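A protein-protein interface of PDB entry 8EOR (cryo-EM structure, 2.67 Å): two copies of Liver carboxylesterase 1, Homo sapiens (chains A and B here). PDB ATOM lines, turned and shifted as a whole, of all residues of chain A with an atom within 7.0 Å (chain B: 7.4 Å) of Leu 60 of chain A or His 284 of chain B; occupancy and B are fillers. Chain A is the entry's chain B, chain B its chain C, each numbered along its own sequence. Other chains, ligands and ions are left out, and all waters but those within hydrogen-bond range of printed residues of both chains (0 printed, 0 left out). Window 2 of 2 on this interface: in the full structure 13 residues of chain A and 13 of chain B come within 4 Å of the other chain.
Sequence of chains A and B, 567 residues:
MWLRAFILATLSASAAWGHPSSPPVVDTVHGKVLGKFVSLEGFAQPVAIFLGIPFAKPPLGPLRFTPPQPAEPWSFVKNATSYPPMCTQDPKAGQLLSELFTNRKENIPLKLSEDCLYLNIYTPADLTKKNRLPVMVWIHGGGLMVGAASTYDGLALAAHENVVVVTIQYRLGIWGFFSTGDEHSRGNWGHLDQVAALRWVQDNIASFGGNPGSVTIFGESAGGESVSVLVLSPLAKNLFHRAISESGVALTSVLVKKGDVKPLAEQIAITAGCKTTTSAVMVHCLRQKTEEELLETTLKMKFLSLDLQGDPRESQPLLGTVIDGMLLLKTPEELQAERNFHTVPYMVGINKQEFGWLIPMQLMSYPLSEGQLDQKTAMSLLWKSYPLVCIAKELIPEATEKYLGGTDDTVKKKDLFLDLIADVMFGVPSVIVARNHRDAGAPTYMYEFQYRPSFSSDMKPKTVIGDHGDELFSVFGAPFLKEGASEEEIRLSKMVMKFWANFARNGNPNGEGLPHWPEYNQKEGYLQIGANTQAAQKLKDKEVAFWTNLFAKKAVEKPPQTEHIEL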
ATOM      1  N   LYS A  57      15.639  21.228 -22.772  1.00  0.00           N
ATOM      2  CA  LYS A  57      17.032  20.840 -22.656  1.00  0.00           C
ATOM      3  C   LYS A  57      17.932  22.071 -22.775  1.00  0.00           C
ATOM      4  O   LYS A  57      17.644  22.983 -23.554  1.00  0.00           O
ATOM      5  CB  LYS A  57      17.372  19.829 -23.742  1.00  0.00           C
ATOM      6  CG  LYS A  57      18.715  19.161 -23.607  1.00  0.00           C
ATOM      7  CD  LYS A  57      18.856  18.084 -24.659  1.00  0.00           C
ATOM      8  CE  LYS A  57      20.169  17.346 -24.537  1.00  0.00           C
ATOM      9  NZ  LYS A  57      20.278  16.278 -25.561  1.00  0.00           N
ATOM     10  N   PRO A  58      19.022  22.131 -22.013  1.00  0.00           N
ATOM     11  CA  PRO A  58      19.927  23.283 -22.109  1.00  0.00           C
ATOM     12  C   PRO A  58      20.437  23.466 -23.528  1.00  0.00           C
ATOM     13  O   PRO A  58      20.938  22.512 -24.140  1.00  0.00           O
ATOM     14  CB  PRO A  58      21.067  22.917 -21.148  1.00  0.00           C
ATOM     15  CG  PRO A  58      20.447  22.010 -20.166  1.00  0.00           C
ATOM     16  CD  PRO A  58      19.405  21.232 -20.909  1.00  0.00           C
ATOM     17  N   PRO A  59      20.342  24.681 -24.089  1.00  0.00           N
ATOM     18  CA  PRO A  59      20.819  24.914 -25.472  1.00  0.00           C
ATOM     19  C   PRO A  59      22.314  25.224 -25.542  1.00  0.00           C
ATOM     20  O   PRO A  59      22.758  26.337 -25.825  1.00  0.00           O
ATOM     21  CB  PRO A  59      19.968  26.101 -25.920  1.00  0.00           C
ATOM     22  CG  PRO A  59      19.750  26.877 -24.665  1.00  0.00           C
ATOM     23  CD  PRO A  59      19.700  25.885 -23.530  1.00  0.00           C
ATOM     24  N   LEU A  60      23.122  24.201 -25.287  1.00  0.00           N
ATOM     25  CA  LEU A  60      24.566  24.339 -25.170  1.00  0.00           C
ATOM     26  C   LEU A  60      25.257  23.690 -26.359  1.00  0.00           C
ATOM     27  O   LEU A  60      24.833  22.633 -26.835  1.00  0.00           O
ATOM     28  CB  LEU A  60      25.065  23.708 -23.870  1.00  0.00           C
ATOM     29  CG  LEU A  60      25.101  24.610 -22.637  1.00  0.00           C
ATOM     30  CD1 LEU A  60      23.857  25.470 -22.528  1.00  0.00           C
ATOM     31  CD2 LEU A  60      25.259  23.762 -21.397  1.00  0.00           C
ATOM     32  N   GLY A  61      26.319  24.334 -26.837  1.00  0.00           N
ATOM     33  CA  GLY A  61      27.127  23.797 -27.904  1.00  0.00           C
ATOM     34  C   GLY A  61      26.366  23.661 -29.208  1.00  0.00           C
ATOM     35  O   GLY A  61      25.869  24.647 -29.761  1.00  0.00           O
ATOM     36  N   PRO A  62      26.265  22.439 -29.736  1.00  0.00           N
ATOM     37  CA  PRO A  62      25.596  22.266 -31.036  1.00  0.00           C
ATOM     38  C   PRO A  62      24.128  22.652 -31.024  1.00  0.00           C
ATOM     39  O   PRO A  62      23.562  22.910 -32.093  1.00  0.00           O
ATOM     40  CB  PRO A  62      25.786  20.772 -31.328  1.00  0.00           C
ATOM     41  CG  PRO A  62      25.946  20.146 -29.999  1.00  0.00           C
ATOM     42  CD  PRO A  62      26.686  21.146 -29.166  1.00  0.00           C
ATOM     43  N   LEU A  63      23.487  22.688 -29.853  1.00  0.00           N
ATOM     44  CA  LEU A  63      22.082  23.068 -29.782  1.00  0.00           C
ATOM     45  C   LEU A  63      21.876  24.570 -29.872  1.00  0.00           C
ATOM     46  O   LEU A  63      20.728  25.014 -29.985  1.00  0.00           O
ATOM     47  CB  LEU A  63      21.457  22.545 -28.488  1.00  0.00           C
ATOM     48  CG  LEU A  63      21.459  21.029 -28.298  1.00  0.00           C
ATOM     49  CD1 LEU A  63      20.627  20.646 -27.092  1.00  0.00           C
ATOM     50  CD2 LEU A  63      20.948  20.325 -29.539  1.00  0.00           C
ATOM     51  N   ARG A  64      22.943  25.360 -29.816  1.00  0.00           N
ATOM     52  CA  ARG A  64      22.821  26.794 -30.028  1.00  0.00           C
ATOM     53  C   ARG A  64      22.261  27.070 -31.416  1.00  0.00           C
ATOM     54  O   ARG A  64      22.705  26.491 -32.410  1.00  0.00           O
ATOM     55  CB  ARG A  64      24.188  27.455 -29.859  1.00  0.00           C
ATOM     56  CG  ARG A  64      24.156  28.960 -29.771  1.00  0.00           C
ATOM     57  CD  ARG A  64      25.553  29.515 -29.568  1.00  0.00           C
ATOM     58  NE  ARG A  64      26.178  29.006 -28.353  1.00  0.00           N
ATOM     59  CZ  ARG A  64      27.457  29.172 -28.042  1.00  0.00           C
ATOM     60  NH1 ARG A  64      28.289  29.806 -28.849  1.00  0.00           N
ATOM     61  NH2 ARG A  64      27.912  28.687 -26.892  1.00  0.00           N
ATOM     62  N   SER A 113      23.759  32.675 -17.632  1.00  0.00           N
ATOM     63  CA  SER A 113      24.055  31.340 -18.127  1.00  0.00           C
ATOM     64  C   SER A 113      23.316  31.110 -19.436  1.00  0.00           C
ATOM     65  O   SER A 113      22.226  31.643 -19.651  1.00  0.00           O
ATOM     66  CB  SER A 113      23.665  30.264 -17.108  1.00  0.00           C
ATOM     67  OG  SER A 113      24.166  28.997 -17.487  1.00  0.00           O
ATOM     68  N   GLU A 114      23.933  30.318 -20.315  1.00  0.00           N
ATOM     69  CA  GLU A 114      23.241  29.868 -21.517  1.00  0.00           C
ATOM     70  C   GLU A 114      22.230  28.781 -21.183  1.00  0.00           C
ATOM     71  O   GLU A 114      21.323  28.501 -21.973  1.00  0.00           O
ATOM     72  CB  GLU A 114      24.248  29.365 -22.546  1.00  0.00           C
ATOM     73  CG  GLU A 114      25.227  30.418 -23.004  1.00  0.00           C
ATOM     74  CD  GLU A 114      26.146  29.917 -24.089  1.00  0.00           C
ATOM     75  OE1 GLU A 114      26.036  28.732 -24.459  1.00  0.00           O
ATOM     76  OE2 GLU A 114      26.979  30.709 -24.573  1.00  0.00           O
ATOM     77  N   ASP A 115      22.386  28.151 -20.024  1.00  0.00           N
ATOM     78  CA  ASP A 115      21.394  27.229 -19.480  1.00  0.00           C
ATOM     79  C   ASP A 115      20.421  28.060 -18.655  1.00  0.00           C
ATOM     80  O   ASP A 115      20.625  28.295 -17.464  1.00  0.00           O
ATOM     81  CB  ASP A 115      22.069  26.151 -18.646  1.00  0.00           C
ATOM     82  CG  ASP A 115      21.093  25.131 -18.117  1.00  0.00           C
ATOM     83  OD1 ASP A 115      19.973  25.042 -18.655  1.00  0.00           O
ATOM     84  OD2 ASP A 115      21.446  24.420 -17.156  1.00  0.00           O
ATOM     85  N   CYS A 116      19.352  28.528 -19.304  1.00  0.00           N
ATOM     86  CA  CYS A 116      18.435  29.477 -18.689  1.00  0.00           C
ATOM     87  C   CYS A 116      16.970  29.197 -19.004  1.00  0.00           C
ATOM     88  O   CYS A 116      16.114  30.019 -18.663  1.00  0.00           O
ATOM     89  CB  CYS A 116      18.781  30.901 -19.131  1.00  0.00           C
ATOM     90  SG  CYS A 116      18.629  31.176 -20.912  1.00  0.00           S
ATOM     91  N   ARG A 287      28.775  28.737 -33.560  1.00  0.00           N
ATOM     92  CA  ARG A 287      28.498  27.660 -32.614  1.00  0.00           C
ATOM     93  C   ARG A 287      29.760  27.217 -31.881  1.00  0.00           C
ATOM     94  O   ARG A 287      29.678  26.586 -30.822  1.00  0.00           O
ATOM     95  CB  ARG A 287      27.859  26.473 -33.328  1.00  0.00           C
ATOM     96  CG  ARG A 287      26.412  26.691 -33.702  1.00  0.00           C
ATOM     97  CD  ARG A 287      25.650  25.388 -33.721  1.00  0.00           C
ATOM     98  NE  ARG A 287      24.286  25.561 -34.206  1.00  0.00           N
ATOM     99  CZ  ARG A 287      23.896  25.357 -35.457  1.00  0.00           C
ATOM    100  NH1 ARG A 287      24.741  24.953 -36.390  1.00  0.00           N
ATOM    101  NH2 ARG A 287      22.624  25.562 -35.780  1.00  0.00           N
ATOM    102  N   LYS A 289      32.018  29.359 -30.752  1.00  0.00           N
ATOM    103  CA  LYS A 289      32.406  30.408 -29.821  1.00  0.00           C
ATOM    104  C   LYS A 289      31.913  30.090 -28.414  1.00  0.00           C
ATOM    105  O   LYS A 289      30.842  29.510 -28.220  1.00  0.00           O
ATOM    106  CB  LYS A 289      31.844  31.753 -30.279  1.00  0.00           C
ATOM    107  CG  LYS A 289      32.302  32.178 -31.661  1.00  0.00           C
ATOM    108  CD  LYS A 289      33.768  32.563 -31.666  1.00  0.00           C
ATOM    109  CE  LYS A 289      34.230  32.970 -33.051  1.00  0.00           C
ATOM    110  NZ  LYS A 289      35.647  33.421 -33.055  1.00  0.00           N
ATOM    111  N   GLU A 291      30.696  31.184 -24.468  1.00  0.00           N
ATOM    112  CA  GLU A 291      29.735  32.159 -23.967  1.00  0.00           C
ATOM    113  C   GLU A 291      30.390  33.519 -23.773  1.00  0.00           C
ATOM    114  O   GLU A 291      29.800  34.555 -24.105  1.00  0.00           O
ATOM    115  CB  GLU A 291      29.129  31.665 -22.653  1.00  0.00           C
ATOM    116  CG  GLU A 291      28.134  32.622 -22.018  1.00  0.00           C
ATOM    117  CD  GLU A 291      27.686  32.170 -20.645  1.00  0.00           C
ATOM    118  OE1 GLU A 291      27.484  30.955 -20.454  1.00  0.00           O
ATOM    119  OE2 GLU A 291      27.547  33.031 -19.752  1.00  0.00           O
ATOM    120  N   PHE B  65      31.162  10.931 -21.107  1.00  0.00           N
ATOM    121  CA  PHE B  65      30.176  11.037 -20.032  1.00  0.00           C
ATOM    122  C   PHE B  65      28.786  10.621 -20.508  1.00  0.00           C
ATOM    123  O   PHE B  65      27.779  11.222 -20.132  1.00  0.00           O
ATOM    124  CB  PHE B  65      30.138  12.452 -19.453  1.00  0.00           C
ATOM    125  CG  PHE B  65      31.484  12.988 -19.065  1.00  0.00           C
ATOM    126  CD1 PHE B  65      32.366  12.221 -18.328  1.00  0.00           C
ATOM    127  CD2 PHE B  65      31.868  14.263 -19.443  1.00  0.00           C
ATOM    128  CE1 PHE B  65      33.600  12.715 -17.977  1.00  0.00           C
ATOM    129  CE2 PHE B  65      33.104  14.758 -19.095  1.00  0.00           C
ATOM    130  CZ  PHE B  65      33.971  13.983 -18.362  1.00  0.00           C
ATOM    131  N   PHE B 178      32.763  10.391 -13.467  1.00  0.00           N
ATOM    132  CA  PHE B 178      32.394  11.765 -13.165  1.00  0.00           C
ATOM    133  C   PHE B 178      30.880  11.879 -13.059  1.00  0.00           C
ATOM    134  O   PHE B 178      30.142  11.380 -13.911  1.00  0.00           O
ATOM    135  CB  PHE B 178      32.918  12.717 -14.237  1.00  0.00           C
ATOM    136  CG  PHE B 178      32.522  14.149 -14.014  1.00  0.00           C
ATOM    137  CD1 PHE B 178      33.227  14.946 -13.130  1.00  0.00           C
ATOM    138  CD2 PHE B 178      31.439  14.695 -14.682  1.00  0.00           C
ATOM    139  CE1 PHE B 178      32.864  16.260 -12.918  1.00  0.00           C
ATOM    140  CE2 PHE B 178      31.071  16.009 -14.472  1.00  0.00           C
ATOM    141  CZ  PHE B 178      31.785  16.791 -13.590  1.00  0.00           C
ATOM    142  N   HIS B 184      22.189  15.261 -15.754  1.00  0.00           N
ATOM    143  CA  HIS B 184      23.106  15.822 -16.742  1.00  0.00           C
ATOM    144  C   HIS B 184      24.394  15.016 -16.821  1.00  0.00           C
ATOM    145  O   HIS B 184      24.965  14.849 -17.905  1.00  0.00           O
ATOM    146  CB  HIS B 184      23.392  17.283 -16.413  1.00  0.00           C
ATOM    147  CG  HIS B 184      22.208  18.175 -16.606  1.00  0.00           C
ATOM    148  ND1 HIS B 184      21.740  19.018 -15.623  1.00  0.00           N
ATOM    149  CD2 HIS B 184      21.384  18.341 -17.667  1.00  0.00           C
ATOM    150  CE1 HIS B 184      20.685  19.672 -16.073  1.00  0.00           C
ATOM    151  NE2 HIS B 184      20.448  19.278 -17.311  1.00  0.00           N
ATOM    152  N   CYS B 274      36.931  25.001 -15.423  1.00  0.00           N
ATOM    153  CA  CYS B 274      35.589  25.207 -15.944  1.00  0.00           C
ATOM    154  C   CYS B 274      34.743  26.033 -14.983  1.00  0.00           C
ATOM    155  O   CYS B 274      35.040  26.148 -13.792  1.00  0.00           O
ATOM    156  CB  CYS B 274      34.913  23.862 -16.195  1.00  0.00           C
ATOM    157  SG  CYS B 274      35.475  23.027 -17.678  1.00  0.00           S
ATOM    158  N   THR B 278      26.315  25.722 -13.355  1.00  0.00           N
ATOM    159  CA  THR B 278      25.260  24.726 -13.434  1.00  0.00           C
ATOM    160  C   THR B 278      25.880  23.378 -13.766  1.00  0.00           C
ATOM    161  O   THR B 278      27.005  23.298 -14.263  1.00  0.00           O
ATOM    162  CB  THR B 278      24.214  25.106 -14.494  1.00  0.00           C
ATOM    163  OG1 THR B 278      23.800  26.462 -14.298  1.00  0.00           O
ATOM    164  CG2 THR B 278      23.002  24.202 -14.408  1.00  0.00           C
ATOM    165  N   SER B 279      25.134  22.310 -13.478  1.00  0.00           N
ATOM    166  CA  SER B 279      25.605  20.975 -13.824  1.00  0.00           C
ATOM    167  C   SER B 279      25.813  20.840 -15.326  1.00  0.00           C
ATOM    168  O   SER B 279      26.837  20.309 -15.776  1.00  0.00           O
ATOM    169  CB  SER B 279      24.613  19.924 -13.330  1.00  0.00           C
ATOM    170  OG  SER B 279      24.544  19.910 -11.916  1.00  0.00           O
ATOM    171  N   ALA B 280      24.858  21.327 -16.119  1.00  0.00           N
ATOM    172  CA  ALA B 280      24.984  21.247 -17.569  1.00  0.00           C
ATOM    173  C   ALA B 280      26.188  22.039 -18.058  1.00  0.00           C
ATOM    174  O   ALA B 280      26.894  21.608 -18.974  1.00  0.00           O
ATOM    175  CB  ALA B 280      23.704  21.748 -18.229  1.00  0.00           C
ATOM    176  N   VAL B 281      26.434  23.206 -17.461  1.00  0.00           N
ATOM    177  CA  VAL B 281      27.587  24.013 -17.848  1.00  0.00           C
ATOM    178  C   VAL B 281      28.881  23.266 -17.560  1.00  0.00           C
ATOM    179  O   VAL B 281      29.796  23.234 -18.391  1.00  0.00           O
ATOM    180  CB  VAL B 281      27.541  25.375 -17.130  1.00  0.00           C
ATOM    181  CG1 VAL B 281      28.885  26.080 -17.213  1.00  0.00           C
ATOM    182  CG2 VAL B 281      26.449  26.242 -17.725  1.00  0.00           C
ATOM    183  N   MET B 282      28.979  22.654 -16.378  1.00  0.00           N
ATOM    184  CA  MET B 282      30.181  21.901 -16.032  1.00  0.00           C
ATOM    185  C   MET B 282      30.394  20.745 -16.998  1.00  0.00           C
ATOM    186  O   MET B 282      31.511  20.519 -17.479  1.00  0.00           O
ATOM    187  CB  MET B 282      30.075  21.379 -14.598  1.00  0.00           C
ATOM    188  CG  MET B 282      30.141  22.453 -13.531  1.00  0.00           C
ATOM    189  SD  MET B 282      30.350  21.779 -11.870  1.00  0.00           S
ATOM    190  CE  MET B 282      28.818  20.879 -11.653  1.00  0.00           C
ATOM    191  N   VAL B 283      29.329  20.000 -17.294  1.00  0.00           N
ATOM    192  CA  VAL B 283      29.456  18.845 -18.176  1.00  0.00           C
ATOM    193  C   VAL B 283      29.879  19.286 -19.570  1.00  0.00           C
ATOM    194  O   VAL B 283      30.788  18.701 -20.175  1.00  0.00           O
ATOM    195  CB  VAL B 283      28.137  18.053 -18.201  1.00  0.00           C
ATOM    196  CG1 VAL B 283      28.240  16.880 -19.151  1.00  0.00           C
ATOM    197  CG2 VAL B 283      27.790  17.564 -16.810  1.00  0.00           C
ATOM    198  N   HIS B 284      29.242  20.333 -20.099  1.00  0.00           N
ATOM    199  CA  HIS B 284      29.605  20.820 -21.423  1.00  0.00           C
ATOM    200  C   HIS B 284      31.054  21.276 -21.458  1.00  0.00           C
ATOM    201  O   HIS B 284      31.801  20.920 -22.375  1.00  0.00           O
ATOM    202  CB  HIS B 284      28.674  21.959 -21.836  1.00  0.00           C
ATOM    203  CG  HIS B 284      28.889  22.434 -23.239  1.00  0.00           C
ATOM    204  ND1 HIS B 284      29.598  23.577 -23.538  1.00  0.00           N
ATOM    205  CD2 HIS B 284      28.497  21.914 -24.425  1.00  0.00           C
ATOM    206  CE1 HIS B 284      29.628  23.744 -24.847  1.00  0.00           C
ATOM    207  NE2 HIS B 284      28.967  22.748 -25.409  1.00  0.00           N
ATOM    208  N   CYS B 285      31.483  22.043 -20.454  1.00  0.00           N
ATOM    209  CA  CYS B 285      32.844  22.563 -20.465  1.00  0.00           C
ATOM    210  C   CYS B 285      33.865  21.441 -20.334  1.00  0.00           C
ATOM    211  O   CYS B 285      34.961  21.524 -20.899  1.00  0.00           O
ATOM    212  CB  CYS B 285      33.022  23.587 -19.348  1.00  0.00           C
ATOM    213  SG  CYS B 285      34.713  24.176 -19.169  1.00  0.00           S
ATOM    214  N   LEU B 286      33.530  20.384 -19.592  1.00  0.00           N
ATOM    215  CA  LEU B 286      34.448  19.257 -19.481  1.00  0.00           C
ATOM    216  C   LEU B 286      34.507  18.457 -20.775  1.00  0.00           C
ATOM    217  O   LEU B 286      35.554  17.899 -21.118  1.00  0.00           O
ATOM    218  CB  LEU B 286      34.038  18.359 -18.314  1.00  0.00           C
ATOM    219  CG  LEU B 286      34.363  18.888 -16.920  1.00  0.00           C
ATOM    220  CD1 LEU B 286      33.737  17.996 -15.878  1.00  0.00           C
ATOM    221  CD2 LEU B 286      35.865  18.986 -16.704  1.00  0.00           C
ATOM    222  N   ARG B 287      33.392  18.381 -21.507  1.00  0.00           N
ATOM    223  CA  ARG B 287      33.404  17.653 -22.773  1.00  0.00           C
ATOM    224  C   ARG B 287      34.273  18.350 -23.813  1.00  0.00           C
ATOM    225  O   ARG B 287      34.685  17.731 -24.800  1.00  0.00           O
ATOM    226  CB  ARG B 287      31.982  17.488 -23.304  1.00  0.00           C
ATOM    227  CG  ARG B 287      31.150  16.486 -22.538  1.00  0.00           C
ATOM    228  CD  ARG B 287      30.113  15.852 -23.437  1.00  0.00           C
ATOM    229  NE  ARG B 287      29.209  14.978 -22.699  1.00  0.00           N
ATOM    230  CZ  ARG B 287      28.024  15.341 -22.229  1.00  0.00           C
ATOM    231  NH1 ARG B 287      27.547  16.561 -22.413  1.00  0.00           N
ATOM    232  NH2 ARG B 287      27.294  14.456 -21.557  1.00  0.00           N
ATOM    233  N   GLN B 288      34.557  19.642 -23.619  1.00  0.00           N
ATOM    234  CA  GLN B 288      35.375  20.363 -24.589  1.00  0.00           C
ATOM    235  C   GLN B 288      36.862  20.188 -24.316  1.00  0.00           C
ATOM    236  O   GLN B 288      37.692  20.530 -25.165  1.00  0.00           O
ATOM    237  CB  GLN B 288      35.015  21.851 -24.586  1.00  0.00           C
ATOM    238  CG  GLN B 288      33.535  22.153 -24.773  1.00  0.00           C
ATOM    239  CD  GLN B 288      32.886  21.314 -25.855  1.00  0.00           C
ATOM    240  OE1 GLN B 288      33.419  21.179 -26.955  1.00  0.00           O
ATOM    241  NE2 GLN B 288      31.730  20.739 -25.547  1.00  0.00           N
ATOM    242  N   LYS B 289      37.222  19.662 -23.148  1.00  0.00           N
ATOM    243  CA  LYS B 289      38.625  19.504 -22.799  1.00  0.00           C
ATOM    244  C   LYS B 289      39.252  18.361 -23.589  1.00  0.00           C
ATOM    245  O   LYS B 289      38.580  17.410 -23.992  1.00  0.00           O
ATOM    246  CB  LYS B 289      38.771  19.241 -21.301  1.00  0.00           C
ATOM    247  CG  LYS B 289      38.195  20.333 -20.421  1.00  0.00           C
ATOM    248  CD  LYS B 289      38.995  21.614 -20.535  1.00  0.00           C
ATOM    249  CE  LYS B 289      38.429  22.708 -19.655  1.00  0.00           C
ATOM    250  NZ  LYS B 289      39.256  23.942 -19.714  1.00  0.00           N
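The backbone NH (N) of Gly 61 of chain A lies close to a ring nitrogen (NE2) of His 284 of chain B (3.4 Å).
The backbone NH (N) of Asp 115 of chain A sits close to the side-chain hydroxyl (OG) of Ser 113 of chain A (3.2 Å). The side-chain amide nitrogen (NE2) of Gln 288 of chain B sits at hydrogen-bond distance from the backbone carbonyl oxygen (O) of His 284 of chain B, at 3.2 Å. SG of Cys 274 of chain B is disulfide-bonded to SG of Cys 285 of chain B (2.0 Å).
His 184 of chain B touches Pro 58 of chain A. Pro 58 of chain A touches Ala 280 of chain B (CG to CB, 3.8 Å). Leu 60 of chain A touches Ala 280 of chain B (CD2 to O, 3.6 Å). CD2 of Leu 60 of chain A touches CB of His 284 of chain B, at 3.9 Å. Ser 113 of chain A touches Val 281 of chain B (OG to CG2, 3.6 Å). CG2 of Thr 278 of chain B touches OD2 of Asp 115 of chain A, 3.2 Å away. Asp 115 of chain A touches Ala 280 of chain B.
Of the printed residues of chain B, Pro 58 of chain A touches His 184 (3.95 Å) and Ala 280 (3.8 Å). Of chain B, only Ala 280 (3.6 Å) and His 284 (3.9 Å) come within 4 Å of Leu 60 of chain A. Of the printed residues of chain B, Ser 113 of chain A touches Val 281. Lys 289 of chain A touches none of the printed residues of chain B. Printed residues of chain A within 4 Å of Ala 280 of chain B: Pro 58, Leu 60 and Asp 115. Printed residues of chain A within 4 Å of Val 281 of chain B: Ser 113 (3.6 Å). Of chain A, only Leu 60 and Gly 61 come within 4 Å of His 284 of chain B. The nearest residue of chain B that does not touch Leu 60 of chain A is Val 281 of chain B (4.1 Å).
Of the 16 printed residues of chain B, 5 touch a printed residue of chain A. Hydrophobic or aromatic side chains of chain B within 4 Å of the printed part of chain A: His 184, Ala 280, Val 281 and His 284. Hydrophobic or aromatic side chains of chain A within 4 Å of the printed part of chain B: Pro 58 and Leu 60. Among the printed residues, 8 pairs touch across the chains. Among the printed residues, no Asp or Glu carboxylate lies within 4 Å of a Lys or Arg side-chain nitrogen of the other chain.
Positions printed for both chains: 287 and 289. Of the 8 pairs that touch across the chains among the printed residues, none has its exchanged pair printed and touching as well.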
